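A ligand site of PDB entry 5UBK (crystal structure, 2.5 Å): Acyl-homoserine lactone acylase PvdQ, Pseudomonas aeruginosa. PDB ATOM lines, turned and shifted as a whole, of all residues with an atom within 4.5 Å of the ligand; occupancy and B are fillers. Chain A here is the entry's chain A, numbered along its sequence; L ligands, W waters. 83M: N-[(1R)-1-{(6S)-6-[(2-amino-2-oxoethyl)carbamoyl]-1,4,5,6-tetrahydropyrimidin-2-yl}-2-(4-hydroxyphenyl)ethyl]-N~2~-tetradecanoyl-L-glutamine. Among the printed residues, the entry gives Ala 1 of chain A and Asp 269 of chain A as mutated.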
ATOM      1  N   ALA A   1      16.782 -14.928   5.109  1.00  0.00           N
ATOM      2  CA  ALA A   1      16.307 -15.880   4.098  1.00  0.00           C
ATOM      3  C   ALA A   1      15.591 -15.186   2.953  1.00  0.00           C
ATOM      4  O   ALA A   1      15.028 -14.095   3.104  1.00  0.00           O
ATOM      5  CB  ALA A   1      15.375 -16.905   4.743  1.00  0.00           C
ATOM      6  N   PRO A  22      17.624 -20.053   2.587  1.00  0.00           N
ATOM      7  CA  PRO A  22      17.743 -19.570   3.964  1.00  0.00           C
ATOM      8  C   PRO A  22      19.167 -19.142   4.301  1.00  0.00           C
ATOM      9  O   PRO A  22      20.149 -19.618   3.721  1.00  0.00           O
ATOM     10  CB  PRO A  22      17.320 -20.779   4.797  1.00  0.00           C
ATOM     11  CG  PRO A  22      17.650 -21.947   3.944  1.00  0.00           C
ATOM     12  CD  PRO A  22      17.412 -21.506   2.524  1.00  0.00           C
ATOM     13  N   HIS A  23      19.273 -18.217   5.266  1.00  0.00           N
ATOM     14  CA  HIS A  23      20.554 -17.680   5.700  1.00  0.00           C
ATOM     15  C   HIS A  23      20.759 -18.066   7.166  1.00  0.00           C
ATOM     16  O   HIS A  23      20.082 -17.534   8.055  1.00  0.00           O
ATOM     17  CB  HIS A  23      20.599 -16.158   5.529  1.00  0.00           C
ATOM     18  CG  HIS A  23      20.332 -15.697   4.131  1.00  0.00           C
ATOM     19  ND1 HIS A  23      19.567 -14.585   3.846  1.00  0.00           N
ATOM     20  CD2 HIS A  23      20.716 -16.200   2.934  1.00  0.00           C
ATOM     21  CE1 HIS A  23      19.499 -14.424   2.539  1.00  0.00           C
ATOM     22  NE2 HIS A  23      20.184 -15.389   1.967  1.00  0.00           N
ATOM     23  N   PHE A  24      21.697 -18.973   7.418  1.00  0.00           N
ATOM     24  CA  PHE A  24      21.911 -19.492   8.762  1.00  0.00           C
ATOM     25  C   PHE A  24      23.409 -19.663   9.018  1.00  0.00           C
ATOM     26  O   PHE A  24      24.205 -19.558   8.084  1.00  0.00           O
ATOM     27  CB  PHE A  24      21.160 -20.815   8.926  1.00  0.00           C
ATOM     28  CG  PHE A  24      20.091 -20.787   9.985  1.00  0.00           C
ATOM     29  CD1 PHE A  24      19.749 -19.601  10.630  1.00  0.00           C
ATOM     30  CD2 PHE A  24      19.429 -21.956  10.349  1.00  0.00           C
ATOM     31  CE1 PHE A  24      18.765 -19.582  11.616  1.00  0.00           C
ATOM     32  CE2 PHE A  24      18.452 -21.939  11.323  1.00  0.00           C
ATOM     33  CZ  PHE A  24      18.123 -20.748  11.958  1.00  0.00           C
ATOM     34  N   PHE A  32      22.897 -26.464   8.750  1.00  0.00           N
ATOM     35  CA  PHE A  32      22.002 -27.337   8.002  1.00  0.00           C
ATOM     36  C   PHE A  32      22.719 -28.619   7.568  1.00  0.00           C
ATOM     37  O   PHE A  32      23.958 -28.675   7.463  1.00  0.00           O
ATOM     38  CB  PHE A  32      21.439 -26.628   6.778  1.00  0.00           C
ATOM     39  CG  PHE A  32      20.188 -25.845   7.034  1.00  0.00           C
ATOM     40  CD1 PHE A  32      19.012 -26.503   7.402  1.00  0.00           C
ATOM     41  CD2 PHE A  32      20.169 -24.466   6.917  1.00  0.00           C
ATOM     42  CE1 PHE A  32      17.845 -25.789   7.636  1.00  0.00           C
ATOM     43  CE2 PHE A  32      19.002 -23.747   7.141  1.00  0.00           C
ATOM     44  CZ  PHE A  32      17.833 -24.411   7.506  1.00  0.00           C
ATOM     45  N   LEU A  50      18.288 -29.211  10.707  1.00  0.00           N
ATOM     46  CA  LEU A  50      19.190 -28.746  11.751  1.00  0.00           C
ATOM     47  C   LEU A  50      19.701 -29.913  12.591  1.00  0.00           C
ATOM     48  O   LEU A  50      19.029 -30.951  12.696  1.00  0.00           O
ATOM     49  CB  LEU A  50      18.464 -27.737  12.647  1.00  0.00           C
ATOM     50  CG  LEU A  50      17.935 -26.516  11.895  1.00  0.00           C
ATOM     51  CD1 LEU A  50      17.412 -25.462  12.853  1.00  0.00           C
ATOM     52  CD2 LEU A  50      19.009 -25.942  10.978  1.00  0.00           C
ATOM     53  N   LEU A  53      17.708 -33.209  14.693  1.00  0.00           N
ATOM     54  CA  LEU A  53      16.284 -33.309  14.417  1.00  0.00           C
ATOM     55  C   LEU A  53      16.011 -34.434  13.421  1.00  0.00           C
ATOM     56  O   LEU A  53      16.561 -34.404  12.306  1.00  0.00           O
ATOM     57  CB  LEU A  53      15.758 -31.992  13.857  1.00  0.00           C
ATOM     58  CG  LEU A  53      15.960 -30.737  14.716  1.00  0.00           C
ATOM     59  CD1 LEU A  53      15.280 -29.539  14.061  1.00  0.00           C
ATOM     60  CD2 LEU A  53      15.417 -30.947  16.113  1.00  0.00           C
ATOM     61  N   ASN A  57      13.509 -30.035   7.597  1.00  0.00           N
ATOM     62  CA  ASN A  57      12.991 -28.704   7.899  1.00  0.00           C
ATOM     63  C   ASN A  57      12.675 -27.901   6.646  1.00  0.00           C
ATOM     64  O   ASN A  57      11.704 -27.134   6.630  1.00  0.00           O
ATOM     65  CB  ASN A  57      13.989 -27.925   8.764  1.00  0.00           C
ATOM     66  CG  ASN A  57      14.186 -28.564  10.135  1.00  0.00           C
ATOM     67  OD1 ASN A  57      15.302 -28.705  10.610  1.00  0.00           O
ATOM     68  ND2 ASN A  57      13.083 -28.950  10.764  1.00  0.00           N
ATOM     69  N   ILE A  58      13.464 -28.067   5.588  1.00  0.00           N
ATOM     70  CA  ILE A  58      13.232 -27.413   4.301  1.00  0.00           C
ATOM     71  C   ILE A  58      13.501 -28.438   3.207  1.00  0.00           C
ATOM     72  O   ILE A  58      14.589 -29.023   3.162  1.00  0.00           O
ATOM     73  CB  ILE A  58      14.118 -26.173   4.106  1.00  0.00           C
ATOM     74  CG1 ILE A  58      13.777 -25.079   5.113  1.00  0.00           C
ATOM     75  CG2 ILE A  58      13.979 -25.640   2.687  1.00  0.00           C
ATOM     76  CD1 ILE A  58      14.692 -23.885   5.050  1.00  0.00           C
ATOM     77  N   HIS A  68      11.302 -21.907   4.505  1.00  0.00           N
ATOM     78  CA  HIS A  68      10.996 -21.023   5.617  1.00  0.00           C
ATOM     79  C   HIS A  68      11.862 -19.764   5.573  1.00  0.00           C
ATOM     80  O   HIS A  68      13.014 -19.792   5.149  1.00  0.00           O
ATOM     81  CB  HIS A  68      11.213 -21.730   6.970  1.00  0.00           C
ATOM     82  CG  HIS A  68      10.405 -22.975   7.137  1.00  0.00           C
ATOM     83  ND1 HIS A  68       9.037 -22.979   7.267  1.00  0.00           N
ATOM     84  CD2 HIS A  68      10.785 -24.272   7.204  1.00  0.00           C
ATOM     85  CE1 HIS A  68       8.604 -24.219   7.404  1.00  0.00           C
ATOM     86  NE2 HIS A  68       9.641 -25.026   7.366  1.00  0.00           N
ATOM     87  N   THR A  69      11.269 -18.664   6.043  1.00  0.00           N
ATOM     88  CA  THR A  69      11.978 -17.415   6.264  1.00  0.00           C
ATOM     89  C   THR A  69      11.602 -16.888   7.644  1.00  0.00           C
ATOM     90  O   THR A  69      10.576 -17.280   8.212  1.00  0.00           O
ATOM     91  CB  THR A  69      11.628 -16.358   5.206  1.00  0.00           C
ATOM     92  OG1 THR A  69      10.272 -15.930   5.353  1.00  0.00           O
ATOM     93  CG2 THR A  69      11.822 -16.919   3.800  1.00  0.00           C
ATOM     94  N   VAL A  70      12.420 -15.992   8.178  1.00  0.00           N
ATOM     95  CA  VAL A  70      12.141 -15.369   9.473  1.00  0.00           C
ATOM     96  C   VAL A  70      11.017 -14.352   9.310  1.00  0.00           C
ATOM     97  O   VAL A  70      11.007 -13.570   8.346  1.00  0.00           O
ATOM     98  CB  VAL A  70      13.407 -14.714  10.044  1.00  0.00           C
ATOM     99  CG1 VAL A  70      13.078 -13.875  11.259  1.00  0.00           C
ATOM    100  CG2 VAL A  70      14.431 -15.763  10.394  1.00  0.00           C
ATOM    101  N   VAL A 158       6.306 -28.991  18.151  1.00  0.00           N
ATOM    102  CA  VAL A 158       7.235 -28.479  17.151  1.00  0.00           C
ATOM    103  C   VAL A 158       7.751 -29.604  16.251  1.00  0.00           C
ATOM    104  O   VAL A 158       7.826 -29.435  15.026  1.00  0.00           O
ATOM    105  CB  VAL A 158       8.388 -27.720  17.836  1.00  0.00           C
ATOM    106  CG1 VAL A 158       9.275 -28.648  18.657  1.00  0.00           C
ATOM    107  CG2 VAL A 158       9.204 -26.985  16.816  1.00  0.00           C
ATOM    108  N   TRP A 162       6.722 -30.535  11.928  1.00  0.00           N
ATOM    109  CA  TRP A 162       7.546 -30.724  10.728  1.00  0.00           C
ATOM    110  C   TRP A 162       7.422 -32.151  10.184  1.00  0.00           C
ATOM    111  O   TRP A 162       7.444 -32.343   8.963  1.00  0.00           O
ATOM    112  CB  TRP A 162       9.014 -30.404  11.018  1.00  0.00           C
ATOM    113  CG  TRP A 162       9.356 -28.978  10.714  1.00  0.00           C
ATOM    114  CD1 TRP A 162       9.487 -28.408   9.480  1.00  0.00           C
ATOM    115  CD2 TRP A 162       9.615 -27.935  11.666  1.00  0.00           C
ATOM    116  NE1 TRP A 162       9.811 -27.080   9.603  1.00  0.00           N
ATOM    117  CE2 TRP A 162       9.887 -26.765  10.934  1.00  0.00           C
ATOM    118  CE3 TRP A 162       9.630 -27.881  13.055  1.00  0.00           C
ATOM    119  CZ2 TRP A 162      10.167 -25.550  11.556  1.00  0.00           C
ATOM    120  CZ3 TRP A 162       9.918 -26.684  13.668  1.00  0.00           C
ATOM    121  CH2 TRP A 162      10.184 -25.531  12.919  1.00  0.00           C
ATOM    122  N   PRO A 185       7.534 -22.479  15.188  1.00  0.00           N
ATOM    123  CA  PRO A 185       7.917 -21.531  16.245  1.00  0.00           C
ATOM    124  C   PRO A 185       8.034 -20.078  15.814  1.00  0.00           C
ATOM    125  O   PRO A 185       7.378 -19.201  16.402  1.00  0.00           O
ATOM    126  CB  PRO A 185       9.287 -22.067  16.704  1.00  0.00           C
ATOM    127  CG  PRO A 185       9.327 -23.487  16.229  1.00  0.00           C
ATOM    128  CD  PRO A 185       8.571 -23.492  14.945  1.00  0.00           C
ATOM    129  N   TRP A 186       8.869 -19.784  14.805  1.00  0.00           N
ATOM    130  CA  TRP A 186       9.172 -18.396  14.509  1.00  0.00           C
ATOM    131  C   TRP A 186       9.637 -18.197  13.069  1.00  0.00           C
ATOM    132  O   TRP A 186      10.549 -17.417  12.800  1.00  0.00           O
ATOM    133  CB  TRP A 186      10.221 -17.844  15.483  1.00  0.00           C
ATOM    134  CG  TRP A 186      11.224 -18.879  15.960  1.00  0.00           C
ATOM    135  CD1 TRP A 186      11.266 -19.481  17.193  1.00  0.00           C
ATOM    136  CD2 TRP A 186      12.330 -19.409  15.221  1.00  0.00           C
ATOM    137  NE1 TRP A 186      12.319 -20.353  17.258  1.00  0.00           N
ATOM    138  CE2 TRP A 186      12.990 -20.335  16.066  1.00  0.00           C
ATOM    139  CE3 TRP A 186      12.825 -19.196  13.936  1.00  0.00           C
ATOM    140  CZ2 TRP A 186      14.124 -21.039  15.654  1.00  0.00           C
ATOM    141  CZ3 TRP A 186      13.945 -19.901  13.524  1.00  0.00           C
ATOM    142  CH2 TRP A 186      14.583 -20.810  14.378  1.00  0.00           C
ATOM    143  N   VAL A 187       8.998 -18.878  12.115  1.00  0.00           N
ATOM    144  CA  VAL A 187       9.340 -18.719  10.709  1.00  0.00           C
ATOM    145  C   VAL A 187       8.072 -18.698   9.867  1.00  0.00           C
ATOM    146  O   VAL A 187       7.079 -19.350  10.183  1.00  0.00           O
ATOM    147  CB  VAL A 187      10.295 -19.820  10.184  1.00  0.00           C
ATOM    148  CG1 VAL A 187      11.708 -19.564  10.634  1.00  0.00           C
ATOM    149  CG2 VAL A 187       9.824 -21.205  10.621  1.00  0.00           C
ATOM    150  N   SER A 268      11.500 -11.911   1.881  1.00  0.00           N
ATOM    151  CA  SER A 268      12.904 -11.803   2.260  1.00  0.00           C
ATOM    152  C   SER A 268      13.036 -11.230   3.663  1.00  0.00           C
ATOM    153  O   SER A 268      13.779 -10.279   3.887  1.00  0.00           O
ATOM    154  CB  SER A 268      13.658 -10.933   1.256  1.00  0.00           C
ATOM    155  OG  SER A 268      13.793 -11.596   0.006  1.00  0.00           O
ATOM    156  N   ASP A 269      12.275 -11.808   4.615  1.00  0.00           N
ATOM    157  CA  ASP A 269      12.335 -11.532   6.050  1.00  0.00           C
ATOM    158  C   ASP A 269      11.618 -10.255   6.461  1.00  0.00           C
ATOM    159  O   ASP A 269      11.843  -9.756   7.567  1.00  0.00           O
ATOM    160  CB  ASP A 269      13.784 -11.501   6.567  1.00  0.00           C
ATOM    161  CG  ASP A 269      14.524 -12.778   6.253  1.00  0.00           C
ATOM    162  OD1 ASP A 269      13.913 -13.866   6.343  1.00  0.00           O
ATOM    163  OD2 ASP A 269      15.724 -12.704   5.890  1.00  0.00           O
ATOM    164  N   ASP A 270      10.757  -9.704   5.611  1.00  0.00           N
ATOM    165  CA  ASP A 270       9.892  -8.603   5.989  1.00  0.00           C
ATOM    166  C   ASP A 270       8.535  -9.133   6.420  1.00  0.00           C
ATOM    167  O   ASP A 270       8.296 -10.347   6.459  1.00  0.00           O
ATOM    168  CB  ASP A 270       9.752  -7.606   4.840  1.00  0.00           C
ATOM    169  CG  ASP A 270      11.074  -6.993   4.424  1.00  0.00           C
ATOM    170  OD1 ASP A 270      11.686  -6.283   5.249  1.00  0.00           O
ATOM    171  OD2 ASP A 270      11.491  -7.224   3.284  1.00  0.00           O
ATOM    172  N   GLY A 295      13.035  -4.426   3.170  1.00  0.00           N
ATOM    173  CA  GLY A 295      14.463  -4.394   3.005  1.00  0.00           C
ATOM    174  C   GLY A 295      14.867  -4.455   1.546  1.00  0.00           C
ATOM    175  O   GLY A 295      14.052  -4.750   0.666  1.00  0.00           O
ATOM    176  N   PRO A 296      16.142  -4.171   1.266  1.00  0.00           N
ATOM    177  CA  PRO A 296      16.573  -4.135  -0.142  1.00  0.00           C
ATOM    178  C   PRO A 296      16.518  -5.491  -0.824  1.00  0.00           C
ATOM    179  O   PRO A 296      16.293  -5.540  -2.047  1.00  0.00           O
ATOM    180  CB  PRO A 296      18.013  -3.617  -0.051  1.00  0.00           C
ATOM    181  CG  PRO A 296      18.466  -4.017   1.329  1.00  0.00           C
ATOM    182  CD  PRO A 296      17.253  -3.926   2.195  1.00  0.00           C
ATOM    183  N   ARG A 297      16.687  -6.588  -0.087  1.00  0.00           N
ATOM    184  CA  ARG A 297      16.581  -7.910  -0.697  1.00  0.00           C
ATOM    185  C   ARG A 297      15.185  -8.150  -1.272  1.00  0.00           C
ATOM    186  O   ARG A 297      15.043  -8.698  -2.371  1.00  0.00           O
ATOM    187  CB  ARG A 297      16.932  -8.994   0.317  1.00  0.00           C
ATOM    188  CG  ARG A 297      18.417  -9.197   0.538  1.00  0.00           C
ATOM    189  CD  ARG A 297      18.713 -10.415   1.403  1.00  0.00           C
ATOM    190  NE  ARG A 297      18.470 -10.164   2.823  1.00  0.00           N
ATOM    191  CZ  ARG A 297      17.491 -10.734   3.530  1.00  0.00           C
ATOM    192  NH1 ARG A 297      16.669 -11.598   2.956  1.00  0.00           N
ATOM    193  NH2 ARG A 297      17.347 -10.440   4.811  1.00  0.00           N
ATOM    194  N   ALA A 298      14.141  -7.746  -0.534  1.00  0.00           N
ATOM    195  CA  ALA A 298      12.787  -7.879  -1.045  1.00  0.00           C
ATOM    196  C   ALA A 298      12.523  -6.933  -2.208  1.00  0.00           C
ATOM    197  O   ALA A 298      11.856  -7.304  -3.172  1.00  0.00           O
ATOM    198  CB  ALA A 298      11.772  -7.642   0.077  1.00  0.00           C
ATOM    199  N   GLY A 456      23.333  -9.072   3.415  1.00  0.00           N
ATOM    200  CA  GLY A 456      21.998  -8.788   2.904  1.00  0.00           C
ATOM    201  C   GLY A 456      21.541  -7.364   3.144  1.00  0.00           C
ATOM    202  O   GLY A 456      20.661  -6.883   2.418  1.00  0.00           O
ATOM    203  N   HIS A 457      22.104  -6.686   4.144  1.00  0.00           N
ATOM    204  CA  HIS A 457      21.721  -5.293   4.399  1.00  0.00           C
ATOM    205  C   HIS A 457      22.008  -4.390   3.208  1.00  0.00           C
ATOM    206  O   HIS A 457      21.398  -3.315   3.095  1.00  0.00           O
ATOM    207  CB  HIS A 457      22.457  -4.760   5.632  1.00  0.00           C
ATOM    208  CG  HIS A 457      21.960  -5.352   6.922  1.00  0.00           C
ATOM    209  ND1 HIS A 457      22.611  -6.378   7.564  1.00  0.00           N
ATOM    210  CD2 HIS A 457      20.889  -5.046   7.685  1.00  0.00           C
ATOM    211  CE1 HIS A 457      21.957  -6.688   8.665  1.00  0.00           C
ATOM    212  NE2 HIS A 457      20.901  -5.899   8.761  1.00  0.00           N
ATOM    213  N   THR A 684      16.391 -29.750  20.963  1.00  0.00           N
ATOM    214  CA  THR A 684      15.127 -29.240  20.422  1.00  0.00           C
ATOM    215  C   THR A 684      14.681 -27.987  21.144  1.00  0.00           C
ATOM    216  O   THR A 684      14.455 -26.939  20.530  1.00  0.00           O
ATOM    217  CB  THR A 684      14.054 -30.321  20.499  1.00  0.00           C
ATOM    218  OG1 THR A 684      14.438 -31.448  19.703  1.00  0.00           O
ATOM    219  CG2 THR A 684      12.719 -29.790  20.004  1.00  0.00           C
ATOM    220  N   LEU A 687      16.654 -24.963  20.373  1.00  0.00           N
ATOM    221  CA  LEU A 687      16.295 -24.318  19.122  1.00  0.00           C
ATOM    222  C   LEU A 687      14.949 -23.609  19.244  1.00  0.00           C
ATOM    223  O   LEU A 687      14.756 -22.524  18.677  1.00  0.00           O
ATOM    224  CB  LEU A 687      16.244 -25.342  17.982  1.00  0.00           C
ATOM    225  CG  LEU A 687      17.559 -26.004  17.544  1.00  0.00           C
ATOM    226  CD1 LEU A 687      17.290 -27.170  16.606  1.00  0.00           C
ATOM    227  CD2 LEU A 687      18.485 -24.996  16.881  1.00  0.00           C
HETATM  228  C8  83M L   1      13.890 -23.876  11.370  1.00  0.00           C
HETATM  229  C9  83M L   1      13.459 -25.087  12.115  1.00  0.00           C
HETATM  230  C16 83M L   1      19.807 -14.560   9.051  1.00  0.00           C
HETATM  231  C6  83M L   1      13.992 -22.864   9.226  1.00  0.00           C
HETATM  232  C5  83M L   1      15.334 -22.220   9.256  1.00  0.00           C
HETATM  233  N23 83M L   1      17.756 -15.760   9.057  1.00  0.00           N
HETATM  234  C1  83M L   1      16.996 -17.940   8.896  1.00  0.00           C
HETATM  235  C2  83M L   1      15.770 -18.561   8.327  1.00  0.00           C
HETATM  236  C3  83M L   1      15.949 -20.041   8.166  1.00  0.00           C
HETATM  237  C4  83M L   1      15.138 -20.747   9.209  1.00  0.00           C
HETATM  238  C7  83M L   1      14.067 -24.181   9.920  1.00  0.00           C
HETATM  239  C13 83M L   1      12.915 -26.941  16.516  1.00  0.00           C
HETATM  240  C12 83M L   1      12.960 -25.726  15.686  1.00  0.00           C
HETATM  241  C11 83M L   1      13.462 -26.068  14.332  1.00  0.00           C
HETATM  242  C10 83M L   1      13.496 -24.793  13.560  1.00  0.00           C
HETATM  243  C14 83M L   1      17.325 -16.668   8.280  1.00  0.00           C
HETATM  244  C15 83M L   1      18.372 -14.564   8.621  1.00  0.00           C
HETATM  245  C17 83M L   1      17.080  -8.556   8.889  1.00  0.00           C
HETATM  246  C18 83M L   1      17.743  -7.386   8.211  1.00  0.00           C
HETATM  247  C19 83M L   1      17.571 -13.421   9.186  1.00  0.00           C
HETATM  248  C20 83M L   1      17.706 -12.178   8.363  1.00  0.00           C
HETATM  249  C21 83M L   1      17.152 -10.934   8.956  1.00  0.00           C
HETATM  250  C22 83M L   1      17.005  -8.360  10.342  1.00  0.00           C
HETATM  251  C23 83M L   1      17.316  -7.290   6.789  1.00  0.00           C
HETATM  252  C24 83M L   1      16.009  -7.418   6.495  1.00  0.00           C
HETATM  253  C25 83M L   1      15.580  -7.349   5.224  1.00  0.00           C
HETATM  254  C26 83M L   1      16.460  -7.155   4.224  1.00  0.00           C
HETATM  255  C27 83M L   1      17.773  -7.021   4.488  1.00  0.00           C
HETATM  256  C28 83M L   1      18.215  -7.081   5.773  1.00  0.00           C
HETATM  257  C29 83M L   1      15.844  -6.188  12.833  1.00  0.00           C
HETATM  258  C32 83M L   1      18.177  -8.454  12.471  1.00  0.00           C
HETATM  259  C33 83M L   1      16.833  -8.446  13.159  1.00  0.00           C
HETATM  260  C34 83M L   1      15.848  -7.614  12.346  1.00  0.00           C
HETATM  261  C35 83M L   1      13.882  -4.857  13.369  1.00  0.00           C
HETATM  262  C36 83M L   1      14.017  -3.384  13.607  1.00  0.00           C
HETATM  263  N24 83M L   1      17.727  -9.806   8.656  1.00  0.00           N
HETATM  264  N30 83M L   1      17.949  -8.754  11.057  1.00  0.00           N
HETATM  265  N31 83M L   1      15.959  -7.808  10.913  1.00  0.00           N
HETATM  266  N32 83M L   1      14.882  -5.365  12.449  1.00  0.00           N
HETATM  267  N40 83M L   1      13.071  -2.713  14.407  1.00  0.00           N
HETATM  268  O15 83M L   1      17.217 -16.504   7.139  1.00  0.00           O
HETATM  269  O17 83M L   1      20.659 -13.986   8.385  1.00  0.00           O
HETATM  270  O18 83M L   1      20.134 -15.139  10.050  1.00  0.00           O
HETATM  271  O22 83M L   1      16.191 -11.001   9.623  1.00  0.00           O
HETATM  272  O29 83M L   1      16.031  -7.080   2.978  1.00  0.00           O
HETATM  273  O30 83M L   1      16.668  -5.787  13.593  1.00  0.00           O
HETATM  274  O39 83M L   1      14.943  -2.796  13.138  1.00  0.00           O
HETATM  275  O   HOH W   1      20.274 -12.539   5.810  1.00  0.00           O
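The backbone NH (N) of Ala 1 lies within hydrogen-bond range of a ring nitrogen (ND1) of His 23 (3.1 Å).
O of Ala 1 lies within hydrogen-bond range of NH1 of Arg 297, 3.0 Å away.
N of Ala 1 sits at hydrogen-bond distance from OD2 of Asp 269 (2.6 Å).
The side-chain carboxylate (OD1) of Asp 270 lies within hydrogen-bond range of the backbone NH (N) of Gly 295 (3.1 Å).
NH2 of Arg 297 is in salt-bridge range of OD2 of Asp 269 (3.0 Å).
The guanidinium group (NH1) of Arg 297 is in hydrogen-bond range of the backbone carbonyl oxygen (O) of Ser 268, at 3.3 Å.
The backbone carbonyl oxygen (O) of Asn 57 is in hydrogen-bond range of a ring nitrogen (NE2) of His 68.
The side-chain amide oxygen (OD1) of Asn 57 lies within hydrogen-bond range of the backbone NH (N) of Leu 50 (3.0 Å).
Water W1 lies within hydrogen-bond range of a ring nitrogen (ND1) of His 23 and an oxygen (O17) of the ligand.
An oxygen (O29) of the ligand lies close to the backbone nitrogen (N) of Pro 296 (3.4 Å).
Merely in contact with the ligand: Gly 295 (3.1 Å), Asp 269 (3.2 Å), Trp 162 (3.4 Å), His 457 (3.5 Å), Gly 456 (3.6 Å), Val 70 (3.6 Å), Phe 24 (3.6 Å), Ser 268 (3.7 Å), Pro 22 (3.7 Å), Val 158 (3.7 Å), His 68 (3.8 Å), Phe 32 (3.8 Å), Val 187 (3.9 Å), Asn 57 (3.9 Å), Leu 53 (3.9 Å) and Leu 687 (3.97 Å).
Within 4 Å of the ligand: Ala 1, Pro 22, His 23, Phe 24, Phe 32, Leu 53, Asn 57, His 68, Val 70, Val 158, Trp 162, Val 187, Ser 268, Asp 269, Gly 295, Pro 296, Arg 297, Gly 456, His 457 and Leu 687.
N of Ala 1 sits at hydrogen-bond distance from O15 of the ligand (2.6 Å).
The backbone NH (N) of His 23 is in hydrogen-bond range of an oxygen (O15) of the ligand, 3.3 Å away.
The backbone carbonyl oxygen (O) of His 23 lies close to a nitrogen (N23) of the ligand, 3.1 Å away.
N of Arg 297 is in hydrogen-bond range of O29 of the ligand.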
